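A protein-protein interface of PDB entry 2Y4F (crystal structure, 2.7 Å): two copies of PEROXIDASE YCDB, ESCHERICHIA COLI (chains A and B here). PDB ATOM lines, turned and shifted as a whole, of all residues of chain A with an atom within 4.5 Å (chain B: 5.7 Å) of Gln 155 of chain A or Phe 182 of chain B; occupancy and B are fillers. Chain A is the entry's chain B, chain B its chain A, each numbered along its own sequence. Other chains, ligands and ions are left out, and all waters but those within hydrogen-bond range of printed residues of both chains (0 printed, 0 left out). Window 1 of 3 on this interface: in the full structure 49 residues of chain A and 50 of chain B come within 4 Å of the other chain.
The side-chain hydroxyl of Ser 322 of chain B sits at hydrogen-bond distance from the side-chain carboxylate of Glu 180 of chain A (2.6 Å).
NE2 of Gln 155 of chain A lies within hydrogen-bond range of OE1 of Glu 180 of chain A.
O of Ser 320 of chain B is in hydrogen-bond range of N of Phe 182 of chain B (2.7 Å).
OG1 of Thr 154 of chain A is in hydrogen-bond range of OD1 of Asp 156 of chain A.
Among the printed residues, merely in contact across the chains: Asp 156 of chain A with Ser 184 of chain B (3.1 Å), Gln 155 of chain A with Phe 182 of chain B (3.2 Å), Ile 159 of chain A with Ser 322 of chain B (3.6 Å), Ile 159 of chain A with Phe 182 of chain B (3.7 Å) and Ile 159 of chain A with Leu 199 of chain B (3.98 Å).
Gln 155 of chain A touches just one residue of chain B: Phe 182.
Of chain A, only Gln 155 and Ile 159 come within 4 Å of Phe 182 of chain B.
Printed residues of chain A within 4 Å of Leu 199 of chain B: Ile 159 (3.98 Å).
Printed residues of chain A within 4 Å of Ser 322 of chain B: Ile 159 and Glu 180.
Printed residues of chain B within 4 Å of Glu 180 of chain A: Ser 322 (2.6 Å).
Gly 181 of chain B touches none of the printed residues of chain A.
The nearest printed residue of chain A that does not touch Phe 182 of chain B is Asp 156 of chain A (4.7 Å).
Of the 14 printed residues of chain B, 4 touch a printed residue of chain A.
Hydrophobic or aromatic side chains of chain B that line the printed part of chain A: Phe 182 and Leu 199.
Along chain B the printed residues that touch a printed residue of chain A span positions 182 to 322.
Of the 8 printed residues of chain A, 4 touch a printed residue of chain B.
Printed residues of chain A that touch a printed residue of chain B: Gln 155, Asp 156, Ile 159 and Glu 180.
Hydrophobic or aromatic side chains of chain A that line the printed part of chain B: Ile 159.
Among the printed residues, no Asp or Glu carboxylate lies within 4 Å of a Lys or Arg side-chain nitrogen of the other chain.
Positions printed for both chains: 40 and 180.
Of the 6 pairs that touch across the chains among the printed residues, none has its exchanged pair printed and touching as well.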
ATOM      1  N   ALA A  40       6.214 -27.925 -29.566  1.00  0.00           N
ATOM      2  CA  ALA A  40       6.825 -26.897 -28.748  1.00  0.00           C
ATOM      3  C   ALA A  40       8.344 -26.948 -28.839  1.00  0.00           C
ATOM      4  O   ALA A  40       8.933 -28.018 -28.939  1.00  0.00           O
ATOM      5  CB  ALA A  40       6.375 -27.041 -27.315  1.00  0.00           C
ATOM      6  N   THR A 154       4.707 -30.679 -25.862  1.00  0.00           N
ATOM      7  CA  THR A 154       4.058 -29.591 -25.139  1.00  0.00           C
ATOM      8  C   THR A 154       5.050 -28.689 -24.432  1.00  0.00           C
ATOM      9  O   THR A 154       6.226 -29.030 -24.248  1.00  0.00           O
ATOM     10  CB  THR A 154       2.989 -30.096 -24.133  1.00  0.00           C
ATOM     11  OG1 THR A 154       3.628 -30.555 -22.937  1.00  0.00           O
ATOM     12  CG2 THR A 154       2.131 -31.229 -24.740  1.00  0.00           C
ATOM     13  N   GLN A 155       4.554 -27.529 -24.033  1.00  0.00           N
ATOM     14  CA  GLN A 155       5.390 -26.513 -23.429  1.00  0.00           C
ATOM     15  C   GLN A 155       5.912 -27.068 -22.110  1.00  0.00           C
ATOM     16  O   GLN A 155       7.097 -26.976 -21.805  1.00  0.00           O
ATOM     17  CB  GLN A 155       4.556 -25.261 -23.191  1.00  0.00           C
ATOM     18  CG  GLN A 155       5.293 -23.977 -23.343  1.00  0.00           C
ATOM     19  CD  GLN A 155       4.407 -22.785 -23.083  1.00  0.00           C
ATOM     20  OE1 GLN A 155       3.182 -22.854 -23.216  1.00  0.00           O
ATOM     21  NE2 GLN A 155       5.024 -21.673 -22.716  1.00  0.00           N
ATOM     22  N   ASP A 156       4.996 -27.670 -21.357  1.00  0.00           N
ATOM     23  CA  ASP A 156       5.275 -28.301 -20.079  1.00  0.00           C
ATOM     24  C   ASP A 156       6.572 -29.088 -20.089  1.00  0.00           C
ATOM     25  O   ASP A 156       7.462 -28.835 -19.272  1.00  0.00           O
ATOM     26  CB  ASP A 156       4.099 -29.199 -19.713  1.00  0.00           C
ATOM     27  CG  ASP A 156       2.774 -28.513 -19.943  1.00  0.00           C
ATOM     28  OD1 ASP A 156       2.489 -28.150 -21.102  1.00  0.00           O
ATOM     29  OD2 ASP A 156       2.024 -28.306 -18.974  1.00  0.00           O
ATOM     30  N   THR A 157       6.686 -30.012 -21.037  1.00  0.00           N
ATOM     31  CA  THR A 157       7.806 -30.952 -21.089  1.00  0.00           C
ATOM     32  C   THR A 157       9.149 -30.228 -21.248  1.00  0.00           C
ATOM     33  O   THR A 157      10.168 -30.625 -20.668  1.00  0.00           O
ATOM     34  CB  THR A 157       7.613 -31.963 -22.241  1.00  0.00           C
ATOM     35  OG1 THR A 157       6.424 -32.719 -22.014  1.00  0.00           O
ATOM     36  CG2 THR A 157       8.803 -32.916 -22.356  1.00  0.00           C
ATOM     37  N   VAL A 158       9.108 -29.159 -22.029  1.00  0.00           N
ATOM     38  CA  VAL A 158      10.248 -28.346 -22.378  1.00  0.00           C
ATOM     39  C   VAL A 158      10.708 -27.543 -21.165  1.00  0.00           C
ATOM     40  O   VAL A 158      11.868 -27.591 -20.754  1.00  0.00           O
ATOM     41  CB  VAL A 158       9.826 -27.461 -23.569  1.00  0.00           C
ATOM     42  CG1 VAL A 158      10.618 -26.234 -23.677  1.00  0.00           C
ATOM     43  CG2 VAL A 158       9.903 -28.270 -24.854  1.00  0.00           C
ATOM     44  N   ILE A 159       9.759 -26.828 -20.588  1.00  0.00           N
ATOM     45  CA  ILE A 159       9.944 -26.079 -19.363  1.00  0.00           C
ATOM     46  C   ILE A 159      10.382 -26.986 -18.214  1.00  0.00           C
ATOM     47  O   ILE A 159      11.140 -26.555 -17.316  1.00  0.00           O
ATOM     48  CB  ILE A 159       8.630 -25.354 -18.991  1.00  0.00           C
ATOM     49  CG1 ILE A 159       8.184 -24.455 -20.162  1.00  0.00           C
ATOM     50  CG2 ILE A 159       8.773 -24.611 -17.654  1.00  0.00           C
ATOM     51  CD1 ILE A 159       7.095 -23.487 -19.841  1.00  0.00           C
ATOM     52  N   GLU A 180      10.936 -19.257 -26.380  1.00  0.00           N
ATOM     53  CA  GLU A 180      10.120 -20.423 -26.593  1.00  0.00           C
ATOM     54  C   GLU A 180       9.272 -20.143 -27.816  1.00  0.00           C
ATOM     55  O   GLU A 180       9.018 -18.975 -28.134  1.00  0.00           O
ATOM     56  CB  GLU A 180       9.265 -20.687 -25.360  1.00  0.00           C
ATOM     57  CG  GLU A 180      10.076 -21.265 -24.189  1.00  0.00           C
ATOM     58  CD  GLU A 180       9.228 -21.559 -22.949  1.00  0.00           C
ATOM     59  OE1 GLU A 180       8.172 -22.225 -23.083  1.00  0.00           O
ATOM     60  OE2 GLU A 180       9.620 -21.125 -21.844  1.00  0.00           O
ATOM     61  N   ALA B  39      -6.596 -24.042 -22.937  1.00  0.00           N
ATOM     62  CA  ALA B  39      -5.169 -24.226 -22.774  1.00  0.00           C
ATOM     63  C   ALA B  39      -4.324 -22.967 -23.006  1.00  0.00           C
ATOM     64  O   ALA B  39      -3.230 -22.855 -22.472  1.00  0.00           O
ATOM     65  CB  ALA B  39      -4.693 -25.355 -23.655  1.00  0.00           C
ATOM     66  N   ALA B  40      -4.813 -22.033 -23.810  1.00  0.00           N
ATOM     67  CA  ALA B  40      -4.028 -20.857 -24.166  1.00  0.00           C
ATOM     68  C   ALA B  40      -4.801 -19.597 -23.799  1.00  0.00           C
ATOM     69  O   ALA B  40      -6.047 -19.547 -23.932  1.00  0.00           O
ATOM     70  CB  ALA B  40      -3.685 -20.864 -25.666  1.00  0.00           C
ATOM     71  N   MET B  41      -4.064 -18.589 -23.339  1.00  0.00           N
ATOM     72  CA  MET B  41      -4.657 -17.305 -23.018  1.00  0.00           C
ATOM     73  C   MET B  41      -3.822 -16.138 -23.548  1.00  0.00           C
ATOM     74  O   MET B  41      -2.669 -16.293 -23.930  1.00  0.00           O
ATOM     75  CB  MET B  41      -4.894 -17.163 -21.514  1.00  0.00           C
ATOM     76  CG  MET B  41      -5.424 -15.790 -21.104  1.00  0.00           C
ATOM     77  SD  MET B  41      -4.881 -15.205 -19.483  1.00  0.00           S
ATOM     78  CE  MET B  41      -6.426 -15.283 -18.573  1.00  0.00           C
ATOM     79  N   GLU B 180       0.872 -13.444 -22.800  1.00  0.00           N
ATOM     80  CA  GLU B 180       0.295 -14.713 -23.210  1.00  0.00           C
ATOM     81  C   GLU B 180       0.550 -15.766 -22.165  1.00  0.00           C
ATOM     82  O   GLU B 180       1.595 -15.746 -21.507  1.00  0.00           O
ATOM     83  CB  GLU B 180       0.903 -15.156 -24.539  1.00  0.00           C
ATOM     84  CG  GLU B 180       0.321 -14.383 -25.726  1.00  0.00           C
ATOM     85  CD  GLU B 180       0.658 -14.993 -27.070  1.00  0.00           C
ATOM     86  OE1 GLU B 180       0.299 -16.166 -27.320  1.00  0.00           O
ATOM     87  OE2 GLU B 180       1.274 -14.280 -27.887  1.00  0.00           O
ATOM     88  N   GLY B 181      -0.398 -16.686 -22.008  1.00  0.00           N
ATOM     89  CA  GLY B 181      -0.301 -17.718 -20.983  1.00  0.00           C
ATOM     90  C   GLY B 181      -0.828 -19.090 -21.366  1.00  0.00           C
ATOM     91  O   GLY B 181      -1.291 -19.320 -22.500  1.00  0.00           O
ATOM     92  N   PHE B 182      -0.769 -20.002 -20.404  1.00  0.00           N
ATOM     93  CA  PHE B 182      -1.196 -21.366 -20.629  1.00  0.00           C
ATOM     94  C   PHE B 182      -1.452 -22.078 -19.316  1.00  0.00           C
ATOM     95  O   PHE B 182      -0.914 -21.700 -18.281  1.00  0.00           O
ATOM     96  CB  PHE B 182      -0.119 -22.127 -21.397  1.00  0.00           C
ATOM     97  CG  PHE B 182       1.152 -22.323 -20.623  1.00  0.00           C
ATOM     98  CD1 PHE B 182       2.128 -21.315 -20.586  1.00  0.00           C
ATOM     99  CD2 PHE B 182       1.377 -23.505 -19.920  1.00  0.00           C
ATOM    100  CE1 PHE B 182       3.323 -21.483 -19.861  1.00  0.00           C
ATOM    101  CE2 PHE B 182       2.568 -23.690 -19.187  1.00  0.00           C
ATOM    102  CZ  PHE B 182       3.544 -22.667 -19.156  1.00  0.00           C
ATOM    103  N   ILE B 183      -2.246 -23.137 -19.361  1.00  0.00           N
ATOM    104  CA  ILE B 183      -2.343 -24.014 -18.202  1.00  0.00           C
ATOM    105  C   ILE B 183      -1.665 -25.315 -18.542  1.00  0.00           C
ATOM    106  O   ILE B 183      -1.473 -25.601 -19.715  1.00  0.00           O
ATOM    107  CB  ILE B 183      -3.783 -24.243 -17.739  1.00  0.00           C
ATOM    108  CG1 ILE B 183      -4.665 -24.609 -18.926  1.00  0.00           C
ATOM    109  CG2 ILE B 183      -4.296 -23.011 -16.990  1.00  0.00           C
ATOM    110  CD1 ILE B 183      -5.991 -25.173 -18.510  1.00  0.00           C
ATOM    111  N   SER B 184      -1.281 -26.064 -17.505  1.00  0.00           N
ATOM    112  CA  SER B 184      -0.617 -27.373 -17.639  1.00  0.00           C
ATOM    113  C   SER B 184      -1.348 -28.338 -18.610  1.00  0.00           C
ATOM    114  O   SER B 184      -2.585 -28.423 -18.600  1.00  0.00           O
ATOM    115  CB  SER B 184      -0.380 -28.005 -16.250  1.00  0.00           C
ATOM    116  OG  SER B 184      -1.523 -27.891 -15.392  1.00  0.00           O
ATOM    117  N   LEU B 199       3.336 -22.979 -12.049  1.00  0.00           N
ATOM    118  CA  LEU B 199       4.749 -23.178 -12.390  1.00  0.00           C
ATOM    119  C   LEU B 199       5.701 -23.305 -11.175  1.00  0.00           C
ATOM    120  O   LEU B 199       6.926 -23.485 -11.329  1.00  0.00           O
ATOM    121  CB  LEU B 199       5.222 -22.114 -13.380  1.00  0.00           C
ATOM    122  CG  LEU B 199       4.986 -22.384 -14.876  1.00  0.00           C
ATOM    123  CD1 LEU B 199       5.451 -21.192 -15.743  1.00  0.00           C
ATOM    124  CD2 LEU B 199       5.667 -23.682 -15.341  1.00  0.00           C
ATOM    125  N   TYR B 319      -3.563 -18.103 -15.240  1.00  0.00           N
ATOM    126  CA  TYR B 319      -2.756 -18.883 -16.186  1.00  0.00           C
ATOM    127  C   TYR B 319      -1.261 -18.749 -15.892  1.00  0.00           C
ATOM    128  O   TYR B 319      -0.837 -17.754 -15.308  1.00  0.00           O
ATOM    129  CB  TYR B 319      -2.997 -18.363 -17.596  1.00  0.00           C
ATOM    130  CG  TYR B 319      -4.210 -18.933 -18.242  1.00  0.00           C
ATOM    131  CD1 TYR B 319      -5.470 -18.498 -17.878  1.00  0.00           C
ATOM    132  CD2 TYR B 319      -4.094 -19.912 -19.229  1.00  0.00           C
ATOM    133  CE1 TYR B 319      -6.596 -19.018 -18.470  1.00  0.00           C
ATOM    134  CE2 TYR B 319      -5.221 -20.446 -19.843  1.00  0.00           C
ATOM    135  CZ  TYR B 319      -6.478 -19.990 -19.451  1.00  0.00           C
ATOM    136  OH  TYR B 319      -7.620 -20.503 -20.028  1.00  0.00           O
ATOM    137  N   SER B 320      -0.479 -19.736 -16.313  1.00  0.00           N
ATOM    138  CA  SER B 320       0.979 -19.672 -16.235  1.00  0.00           C
ATOM    139  C   SER B 320       1.541 -18.940 -17.447  1.00  0.00           C
ATOM    140  O   SER B 320       0.950 -19.008 -18.543  1.00  0.00           O
ATOM    141  CB  SER B 320       1.605 -21.069 -16.209  1.00  0.00           C
ATOM    142  OG  SER B 320       1.196 -21.809 -15.073  1.00  0.00           O
ATOM    143  N   TYR B 321       2.675 -18.254 -17.243  1.00  0.00           N
ATOM    144  CA  TYR B 321       3.481 -17.714 -18.340  1.00  0.00           C
ATOM    145  C   TYR B 321       4.959 -18.084 -18.239  1.00  0.00           C
ATOM    146  O   TYR B 321       5.489 -18.300 -17.157  1.00  0.00           O
ATOM    147  CB  TYR B 321       3.314 -16.190 -18.476  1.00  0.00           C
ATOM    148  CG  TYR B 321       4.072 -15.327 -17.477  1.00  0.00           C
ATOM    149  CD1 TYR B 321       5.404 -15.002 -17.683  1.00  0.00           C
ATOM    150  CD2 TYR B 321       3.424 -14.800 -16.342  1.00  0.00           C
ATOM    151  CE1 TYR B 321       6.099 -14.190 -16.761  1.00  0.00           C
ATOM    152  CE2 TYR B 321       4.087 -13.983 -15.431  1.00  0.00           C
ATOM    153  CZ  TYR B 321       5.430 -13.681 -15.639  1.00  0.00           C
ATOM    154  OH  TYR B 321       6.097 -12.869 -14.738  1.00  0.00           O
ATOM    155  N   SER B 322       5.614 -18.138 -19.384  1.00  0.00           N
ATOM    156  CA  SER B 322       7.027 -18.424 -19.450  1.00  0.00           C
ATOM    157  C   SER B 322       7.616 -17.667 -20.647  1.00  0.00           C
ATOM    158  O   SER B 322       7.290 -17.976 -21.793  1.00  0.00           O
ATOM    159  CB  SER B 322       7.210 -19.914 -19.629  1.00  0.00           C
ATOM    160  OG  SER B 322       8.569 -20.254 -19.604  1.00  0.00           O
ATOM    161  N   LEU B 336      -0.147 -15.298 -14.775  1.00  0.00           N
ATOM    162  CA  LEU B 336      -1.109 -14.280 -15.200  1.00  0.00           C
ATOM    163  C   LEU B 336      -2.353 -14.491 -14.346  1.00  0.00           C
ATOM    164  O   LEU B 336      -3.169 -15.382 -14.640  1.00  0.00           O
ATOM    165  CB  LEU B 336      -1.444 -14.415 -16.695  1.00  0.00           C
ATOM    166  CG  LEU B 336      -0.239 -14.493 -17.637  1.00  0.00           C
ATOM    167  CD1 LEU B 336      -0.698 -14.579 -19.087  1.00  0.00           C
ATOM    168  CD2 LEU B 336       0.691 -13.294 -17.424  1.00  0.00           C
